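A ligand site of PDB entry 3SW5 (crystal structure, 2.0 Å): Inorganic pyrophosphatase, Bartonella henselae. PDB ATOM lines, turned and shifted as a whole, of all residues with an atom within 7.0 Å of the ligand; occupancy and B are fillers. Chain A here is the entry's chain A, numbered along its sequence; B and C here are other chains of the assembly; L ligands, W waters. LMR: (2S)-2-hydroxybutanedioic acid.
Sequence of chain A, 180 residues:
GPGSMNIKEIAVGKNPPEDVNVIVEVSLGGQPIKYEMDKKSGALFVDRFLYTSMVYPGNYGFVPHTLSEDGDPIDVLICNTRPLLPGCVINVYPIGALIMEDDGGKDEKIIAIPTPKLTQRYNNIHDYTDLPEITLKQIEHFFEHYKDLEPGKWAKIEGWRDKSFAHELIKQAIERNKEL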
ATOM      1  N   LEU A  28      17.272  23.830  18.167  1.00  0.00           N
ATOM      2  CA  LEU A  28      17.215  22.987  19.329  1.00  0.00           C
ATOM      3  C   LEU A  28      18.510  23.149  20.132  1.00  0.00           C
ATOM      4  O   LEU A  28      19.622  23.212  19.565  1.00  0.00           O
ATOM      5  CB  LEU A  28      17.109  21.564  18.845  1.00  0.00           C
ATOM      6  CG  LEU A  28      17.107  20.406  19.812  1.00  0.00           C
ATOM      7  CD1 LEU A  28      16.705  19.168  18.972  1.00  0.00           C
ATOM      8  CD2 LEU A  28      18.484  20.201  20.459  1.00  0.00           C
ATOM      9  N   ASN A  59      13.623  22.017  17.215  1.00  0.00           N
ATOM     10  CA  ASN A  59      13.815  23.211  16.359  1.00  0.00           C
ATOM     11  C   ASN A  59      12.495  23.838  16.196  1.00  0.00           C
ATOM     12  O   ASN A  59      11.498  23.127  16.055  1.00  0.00           O
ATOM     13  CB  ASN A  59      14.388  22.818  15.008  1.00  0.00           C
ATOM     14  CG  ASN A  59      15.777  22.307  15.108  1.00  0.00           C
ATOM     15  OD1 ASN A  59      16.737  23.091  15.328  1.00  0.00           O
ATOM     16  ND2 ASN A  59      15.923  20.979  14.975  1.00  0.00           N
ATOM     17  N   CYS A  79      10.545  17.890  16.313  1.00  0.00           N
ATOM     18  CA  CYS A  79      11.207  17.109  17.361  1.00  0.00           C
ATOM     19  C   CYS A  79      12.210  16.102  16.783  1.00  0.00           C
ATOM     20  O   CYS A  79      12.142  14.876  17.040  1.00  0.00           O
ATOM     21  CB  CYS A  79      10.182  16.424  18.265  1.00  0.00           C
ATOM     22  SG  CYS A  79       9.143  15.392  17.383  1.00  0.00           S
ATOM     23  N   ASN A  80      13.162  16.641  16.028  1.00  0.00           N
ATOM     24  CA  ASN A  80      14.327  15.903  15.608  1.00  0.00           C
ATOM     25  C   ASN A  80      15.423  16.172  16.640  1.00  0.00           C
ATOM     26  O   ASN A  80      15.174  16.868  17.647  1.00  0.00           O
ATOM     27  CB  ASN A  80      14.718  16.238  14.166  1.00  0.00           C
ATOM     28  CG  ASN A  80      15.281  17.625  14.035  1.00  0.00           C
ATOM     29  OD1 ASN A  80      14.641  18.599  14.422  1.00  0.00           O
ATOM     30  ND2 ASN A  80      16.502  17.726  13.476  1.00  0.00           N
ATOM     31  N   THR A  81      16.623  15.621  16.421  1.00  0.00           N
ATOM     32  CA  THR A  81      17.658  15.712  17.438  1.00  0.00           C
ATOM     33  C   THR A  81      18.790  16.665  17.042  1.00  0.00           C
ATOM     34  O   THR A  81      19.603  17.011  17.893  1.00  0.00           O
ATOM     35  CB  THR A  81      18.225  14.358  17.826  1.00  0.00           C
ATOM     36  OG1 THR A  81      19.046  13.837  16.764  1.00  0.00           O
ATOM     37  CG2 THR A  81      17.072  13.355  18.182  1.00  0.00           C
ATOM     38  N   ARG A  82      18.834  17.107  15.778  1.00  0.00           N
ATOM     39  CA  ARG A  82      19.958  17.908  15.321  1.00  0.00           C
ATOM     40  C   ARG A  82      19.512  19.371  15.163  1.00  0.00           C
ATOM     41  O   ARG A  82      18.479  19.628  14.624  1.00  0.00           O
ATOM     42  CB  ARG A  82      20.525  17.374  13.985  1.00  0.00           C
ATOM     43  CG  ARG A  82      21.070  15.952  14.024  1.00  0.00           C
ATOM     44  CD  ARG A  82      21.600  15.572  12.636  1.00  0.00           C
ATOM     45  NE  ARG A  82      21.993  14.175  12.534  1.00  0.00           N
ATOM     46  CZ  ARG A  82      23.148  13.690  13.007  1.00  0.00           C
ATOM     47  NH1 ARG A  82      24.016  14.478  13.612  1.00  0.00           N
ATOM     48  NH2 ARG A  82      23.404  12.410  12.891  1.00  0.00           N
ATOM     49  N   PRO A  83      20.348  20.333  15.581  1.00  0.00           N
ATOM     50  CA  PRO A  83      20.043  21.744  15.405  1.00  0.00           C
ATOM     51  C   PRO A  83      20.092  22.192  13.973  1.00  0.00           C
ATOM     52  O   PRO A  83      21.009  21.800  13.219  1.00  0.00           O
ATOM     53  CB  PRO A  83      21.144  22.470  16.200  1.00  0.00           C
ATOM     54  CG  PRO A  83      22.261  21.523  16.282  1.00  0.00           C
ATOM     55  CD  PRO A  83      21.636  20.135  16.273  1.00  0.00           C
ATOM     56  N   LEU A  84      19.110  23.014  13.605  1.00  0.00           N
ATOM     57  CA  LEU A  84      18.983  23.543  12.270  1.00  0.00           C
ATOM     58  C   LEU A  84      19.334  25.007  12.329  1.00  0.00           C
ATOM     59  O   LEU A  84      19.188  25.644  13.356  1.00  0.00           O
ATOM     60  CB  LEU A  84      17.575  23.358  11.754  1.00  0.00           C
ATOM     61  CG  LEU A  84      17.196  21.875  11.627  1.00  0.00           C
ATOM     62  CD1 LEU A  84      15.689  21.671  11.393  1.00  0.00           C
ATOM     63  CD2 LEU A  84      18.028  21.223  10.511  1.00  0.00           C
ATOM     64  N   PRO A 114      10.764  15.572  10.581  1.00  0.00           N
ATOM     65  CA  PRO A 114      11.221  15.611   9.195  1.00  0.00           C
ATOM     66  C   PRO A 114      10.595  14.540   8.347  1.00  0.00           C
ATOM     67  O   PRO A 114      10.380  13.447   8.824  1.00  0.00           O
ATOM     68  CB  PRO A 114      12.740  15.419   9.332  1.00  0.00           C
ATOM     69  CG  PRO A 114      13.046  15.960  10.692  1.00  0.00           C
ATOM     70  CD  PRO A 114      11.903  15.567  11.526  1.00  0.00           C
ATOM     71  N   LEU A 118      13.965  13.580   3.693  1.00  0.00           N
ATOM     72  CA  LEU A 118      15.063  14.244   4.401  1.00  0.00           C
ATOM     73  C   LEU A 118      15.820  13.254   5.291  1.00  0.00           C
ATOM     74  O   LEU A 118      17.040  13.341   5.417  1.00  0.00           O
ATOM     75  CB  LEU A 118      14.588  15.409   5.248  1.00  0.00           C
ATOM     76  CG  LEU A 118      13.700  16.533   4.684  1.00  0.00           C
ATOM     77  CD1 LEU A 118      13.746  17.755   5.606  1.00  0.00           C
ATOM     78  CD2 LEU A 118      14.053  16.931   3.243  1.00  0.00           C
ATOM     79  N   THR A 119      15.096  12.309   5.898  1.00  0.00           N
ATOM     80  CA  THR A 119      15.690  11.302   6.744  1.00  0.00           C
ATOM     81  C   THR A 119      14.801  10.100   6.953  1.00  0.00           C
ATOM     82  O   THR A 119      13.594  10.230   7.146  1.00  0.00           O
ATOM     83  CB  THR A 119      16.089  11.850   8.123  1.00  0.00           C
ATOM     84  OG1 THR A 119      16.517  10.770   8.969  1.00  0.00           O
ATOM     85  CG2 THR A 119      14.943  12.626   8.795  1.00  0.00           C
ATOM     86  N   GLN A 120      15.424   8.931   6.958  1.00  0.00           N
ATOM     87  CA  GLN A 120      14.759   7.658   7.181  1.00  0.00           C
ATOM     88  C   GLN A 120      14.670   7.295   8.672  1.00  0.00           C
ATOM     89  O   GLN A 120      14.118   6.259   9.038  1.00  0.00           O
ATOM     90  CB  GLN A 120      15.507   6.577   6.415  1.00  0.00           C
ATOM     91  CG  GLN A 120      15.482   6.755   4.908  1.00  0.00           C
ATOM     92  CD  GLN A 120      14.164   6.316   4.322  1.00  0.00           C
ATOM     93  OE1 GLN A 120      13.743   5.177   4.535  1.00  0.00           O
ATOM     94  NE2 GLN A 120      13.502   7.198   3.594  1.00  0.00           N
ATOM     95  N   ARG A 121      15.182   8.152   9.540  1.00  0.00           N
ATOM     96  CA  ARG A 121      15.231   7.886  10.963  1.00  0.00           C
ATOM     97  C   ARG A 121      13.857   7.796  11.675  1.00  0.00           C
ATOM     98  O   ARG A 121      13.762   7.178  12.746  1.00  0.00           O
ATOM     99  CB  ARG A 121      16.038   9.017  11.631  1.00  0.00           C
ATOM    100  CG  ARG A 121      16.482   8.796  13.061  1.00  0.00           C
ATOM    101  CD  ARG A 121      17.856   8.194  13.140  1.00  0.00           C
ATOM    102  NE  ARG A 121      18.900   9.089  12.629  1.00  0.00           N
ATOM    103  CZ  ARG A 121      20.092   8.669  12.204  1.00  0.00           C
ATOM    104  NH1 ARG A 121      20.979   9.541  11.761  1.00  0.00           N
ATOM    105  NH2 ARG A 121      20.434   7.395  12.232  1.00  0.00           N
ATOM    106  N   TYR A 122      12.824   8.433  11.104  1.00  0.00           N
ATOM    107  CA  TYR A 122      11.486   8.544  11.725  1.00  0.00           C
ATOM    108  C   TYR A 122      10.411   7.754  10.958  1.00  0.00           C
ATOM    109  O   TYR A 122       9.222   8.082  11.036  1.00  0.00           O
ATOM    110  CB  TYR A 122      11.081  10.037  11.825  1.00  0.00           C
ATOM    111  CG  TYR A 122      12.049  10.769  12.698  1.00  0.00           C
ATOM    112  CD1 TYR A 122      12.001  10.585  14.070  1.00  0.00           C
ATOM    113  CD2 TYR A 122      13.083  11.513  12.162  1.00  0.00           C
ATOM    114  CE1 TYR A 122      12.919  11.168  14.900  1.00  0.00           C
ATOM    115  CE2 TYR A 122      14.027  12.115  12.993  1.00  0.00           C
ATOM    116  CZ  TYR A 122      13.921  11.940  14.369  1.00  0.00           C
ATOM    117  OH  TYR A 122      14.819  12.478  15.251  1.00  0.00           O
ATOM    118  N   GLN B  31      27.421  19.322  11.639  1.00  0.00           N
ATOM    119  CA  GLN B  31      26.206  18.515  11.462  1.00  0.00           C
ATOM    120  C   GLN B  31      26.075  18.032  10.010  1.00  0.00           C
ATOM    121  O   GLN B  31      26.403  18.775   9.080  1.00  0.00           O
ATOM    122  CB  GLN B  31      24.974  19.322  11.861  1.00  0.00           C
ATOM    123  CG  GLN B  31      24.842  19.583  13.376  1.00  0.00           C
ATOM    124  CD  GLN B  31      24.636  18.279  14.153  1.00  0.00           C
ATOM    125  OE1 GLN B  31      23.849  17.447  13.757  1.00  0.00           O
ATOM    126  NE2 GLN B  31      25.357  18.126  15.265  1.00  0.00           N
ATOM    127  N   PRO B  32      25.611  16.780   9.820  1.00  0.00           N
ATOM    128  CA  PRO B  32      25.482  16.269   8.470  1.00  0.00           C
ATOM    129  C   PRO B  32      24.199  16.779   7.837  1.00  0.00           C
ATOM    130  O   PRO B  32      23.273  16.004   7.550  1.00  0.00           O
ATOM    131  CB  PRO B  32      25.429  14.757   8.700  1.00  0.00           C
ATOM    132  CG  PRO B  32      24.744  14.624   9.991  1.00  0.00           C
ATOM    133  CD  PRO B  32      25.229  15.775  10.820  1.00  0.00           C
ATOM    134  N   ILE B  33      24.142  18.095   7.612  1.00  0.00           N
ATOM    135  CA  ILE B  33      22.924  18.715   7.085  1.00  0.00           C
ATOM    136  C   ILE B  33      23.188  19.343   5.736  1.00  0.00           C
ATOM    137  O   ILE B  33      23.950  20.313   5.622  1.00  0.00           O
ATOM    138  CB  ILE B  33      22.289  19.796   8.018  1.00  0.00           C
ATOM    139  CG1 ILE B  33      21.970  19.210   9.390  1.00  0.00           C
ATOM    140  CG2 ILE B  33      20.997  20.329   7.383  1.00  0.00           C
ATOM    141  CD1 ILE B  33      21.641  20.263  10.505  1.00  0.00           C
ATOM    142  N   PHE B  49      19.227  15.154   5.474  1.00  0.00           N
ATOM    143  CA  PHE B  49      20.309  14.848   6.381  1.00  0.00           C
ATOM    144  C   PHE B  49      21.088  13.789   5.632  1.00  0.00           C
ATOM    145  O   PHE B  49      20.495  13.029   4.853  1.00  0.00           O
ATOM    146  CB  PHE B  49      19.791  14.332   7.718  1.00  0.00           C
ATOM    147  CG  PHE B  49      18.893  15.294   8.419  1.00  0.00           C
ATOM    148  CD1 PHE B  49      17.526  15.327   8.151  1.00  0.00           C
ATOM    149  CD2 PHE B  49      19.401  16.191   9.336  1.00  0.00           C
ATOM    150  CE1 PHE B  49      16.713  16.201   8.803  1.00  0.00           C
ATOM    151  CE2 PHE B  49      18.571  17.067   9.986  1.00  0.00           C
ATOM    152  CZ  PHE B  49      17.241  17.076   9.730  1.00  0.00           C
ATOM    153  N   LEU B  50      22.401  13.747   5.795  1.00  0.00           N
ATOM    154  CA  LEU B  50      23.161  12.745   5.092  1.00  0.00           C
ATOM    155  C   LEU B  50      22.684  11.352   5.541  1.00  0.00           C
ATOM    156  O   LEU B  50      22.437  11.134   6.743  1.00  0.00           O
ATOM    157  CB  LEU B  50      24.653  12.911   5.314  1.00  0.00           C
ATOM    158  CG  LEU B  50      25.269  14.135   4.648  1.00  0.00           C
ATOM    159  CD1 LEU B  50      26.788  14.067   4.718  1.00  0.00           C
ATOM    160  CD2 LEU B  50      24.765  14.274   3.172  1.00  0.00           C
ATOM    161  N   TYR B  51      22.565  10.433   4.594  1.00  0.00           N
ATOM    162  CA  TYR B  51      22.178   9.041   4.903  1.00  0.00           C
ATOM    163  C   TYR B  51      23.304   8.164   5.469  1.00  0.00           C
ATOM    164  O   TYR B  51      23.068   7.071   5.995  1.00  0.00           O
ATOM    165  CB  TYR B  51      21.565   8.388   3.680  1.00  0.00           C
ATOM    166  CG  TYR B  51      20.151   8.796   3.397  1.00  0.00           C
ATOM    167  CD1 TYR B  51      19.162   7.830   3.097  1.00  0.00           C
ATOM    168  CD2 TYR B  51      19.770  10.126   3.464  1.00  0.00           C
ATOM    169  CE1 TYR B  51      17.849   8.203   2.812  1.00  0.00           C
ATOM    170  CE2 TYR B  51      18.475  10.510   3.178  1.00  0.00           C
ATOM    171  CZ  TYR B  51      17.523   9.548   2.852  1.00  0.00           C
ATOM    172  OH  TYR B  51      16.218   9.966   2.612  1.00  0.00           O
ATOM    173  N   THR C  81      22.197   9.761  21.047  1.00  0.00           N
ATOM    174  CA  THR C  81      22.369  10.899  20.127  1.00  0.00           C
ATOM    175  C   THR C  81      23.303  12.011  20.653  1.00  0.00           C
ATOM    176  O   THR C  81      23.672  12.922  19.883  1.00  0.00           O
ATOM    177  CB  THR C  81      21.023  11.442  19.736  1.00  0.00           C
ATOM    178  OG1 THR C  81      20.489  12.181  20.833  1.00  0.00           O
ATOM    179  CG2 THR C  81      20.033  10.259  19.414  1.00  0.00           C
ATOM    180  N   ILE C 134      17.622   2.627   9.243  1.00  0.00           N
ATOM    181  CA  ILE C 134      18.737   3.446   8.760  1.00  0.00           C
ATOM    182  C   ILE C 134      19.898   3.569   9.798  1.00  0.00           C
ATOM    183  O   ILE C 134      21.065   3.703   9.422  1.00  0.00           O
ATOM    184  CB  ILE C 134      18.260   4.826   8.276  1.00  0.00           C
ATOM    185  CG1 ILE C 134      19.350   5.490   7.417  1.00  0.00           C
ATOM    186  CG2 ILE C 134      17.794   5.703   9.474  1.00  0.00           C
ATOM    187  CD1 ILE C 134      19.518   4.845   6.003  1.00  0.00           C
ATOM    188  N   THR C 135      19.580   3.482  11.086  1.00  0.00           N
ATOM    189  CA  THR C 135      20.644   3.566  12.088  1.00  0.00           C
ATOM    190  C   THR C 135      21.553   2.391  11.977  1.00  0.00           C
ATOM    191  O   THR C 135      22.767   2.531  12.016  1.00  0.00           O
ATOM    192  CB  THR C 135      20.103   3.681  13.528  1.00  0.00           C
ATOM    193  OG1 THR C 135      19.362   4.900  13.638  1.00  0.00           O
ATOM    194  CG2 THR C 135      21.255   3.648  14.584  1.00  0.00           C
ATOM    195  N   GLN C 138      23.758   2.650   8.819  1.00  0.00           N
ATOM    196  CA  GLN C 138      24.828   3.612   9.014  1.00  0.00           C
ATOM    197  C   GLN C 138      25.937   3.054   9.854  1.00  0.00           C
ATOM    198  O   GLN C 138      27.089   3.307   9.572  1.00  0.00           O
ATOM    199  CB  GLN C 138      24.307   4.880   9.673  1.00  0.00           C
ATOM    200  CG  GLN C 138      23.435   5.713   8.732  1.00  0.00           C
ATOM    201  CD  GLN C 138      22.671   6.800   9.483  1.00  0.00           C
ATOM    202  OE1 GLN C 138      22.666   6.818  10.706  1.00  0.00           O
ATOM    203  NE2 GLN C 138      22.040   7.698   8.749  1.00  0.00           N
HETATM  204  C1  LMR L   1      17.659  14.127  13.551  1.00  0.00           C
HETATM  205  O1A LMR L   1      16.709  13.815  14.338  1.00  0.00           O
HETATM  206  O1B LMR L   1      17.950  15.352  13.352  1.00  0.00           O
HETATM  207  C2  LMR L   1      18.430  13.034  12.873  1.00  0.00           C
HETATM  208  O2  LMR L   1      17.999  11.727  13.211  1.00  0.00           O
HETATM  209  C3  LMR L   1      18.326  13.195  11.375  1.00  0.00           C
HETATM  210  C4  LMR L   1      19.345  12.325  10.700  1.00  0.00           C
HETATM  211  O4A LMR L   1      18.963  11.450   9.861  1.00  0.00           O
HETATM  212  O4B LMR L   1      20.553  12.442  10.991  1.00  0.00           O
HETATM  213  O   HOH W   1      20.229   9.922   8.086  1.00  0.00           O
HETATM  214  O   HOH W   2      18.533  11.383  15.748  1.00  0.00           O
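OH of Tyr 122 is in hydrogen-bond range of O1A of the ligand (2.5 Å). The side-chain hydroxyl of Thr 119 is in hydrogen-bond range of an oxygen (O4A) of the ligand (2.7 Å). O1B of the ligand sits at hydrogen-bond distance from N of Arg 82, at 3.1 Å. The guanidinium group of Arg 82 lies within salt-bridge range of an oxygen (O4B) of the ligand (2.7 Å). An oxygen (O1A) of the ligand sits at hydrogen-bond distance from the backbone NH of Thr 81 of chain A (2.8 Å). OG1 of Thr 81 of chain A sits at hydrogen-bond distance from O1A of the ligand, 3.4 Å away. The side-chain amide nitrogen (ND2) of Asn 80 sits at hydrogen-bond distance from an oxygen (O1B) of the ligand (2.8 Å). The guanidinium group of Arg 121 lies within salt-bridge range of an oxygen (O4B) of the ligand, 3.0 Å away.
Phe 49 of chain B touches the ligand (CB to C4, 3.6 Å). Hydrophobic or aromatic side chains within 4 Å of the ligand: Tyr 122 and Phe 49 of chain B. Seven residues have an atom within 4 Å of the ligand: Asn 80, Thr 81 of chain A, Arg 82, Thr 119, Arg 121, Tyr 122 and Phe 49 of chain B.
Water W2 lies within hydrogen-bond range of an oxygen (O2) of the ligand (2.6 Å) and the side-chain hydroxyl (OG1) of Thr 81 of chain A (2.7 Å). Water W1 lies within hydrogen-bond range of an oxygen (O4A) of the ligand, the backbone carbonyl oxygen (O) of Leu 50 of chain B and the side-chain amide nitrogen (NE2) of Gln 138 of chain C.
N of Arg 121 sits at hydrogen-bond distance from OG1 of Thr 119. The backbone carbonyl oxygen (O) of Arg 82 is in hydrogen-bond range of the side-chain amide nitrogen (ND2) of Asn 80. The backbone carbonyl oxygen (O) of Arg 82 is in hydrogen-bond range of the side-chain amide nitrogen (ND2) of Asn 59, 2.9 Å away. NH1 of Arg 82 lies within hydrogen-bond range of OE1 of Gln 31 of chain B (3.0 Å). OD1 of Asn 80 lies within hydrogen-bond range of ND2 of Asn 59, at 2.8 Å. OE1 of Gln 138 of chain C is in hydrogen-bond range of NH2 of Arg 121 (2.8 Å). The guanidinium group (NH2) of Arg 121 is in hydrogen-bond range of the side-chain hydroxyl (OG1) of Thr 135 of chain C (3.1 Å). The backbone NH of Phe 49 of chain B is in hydrogen-bond range of the backbone carbonyl oxygen of Leu 118 (2.8 Å).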
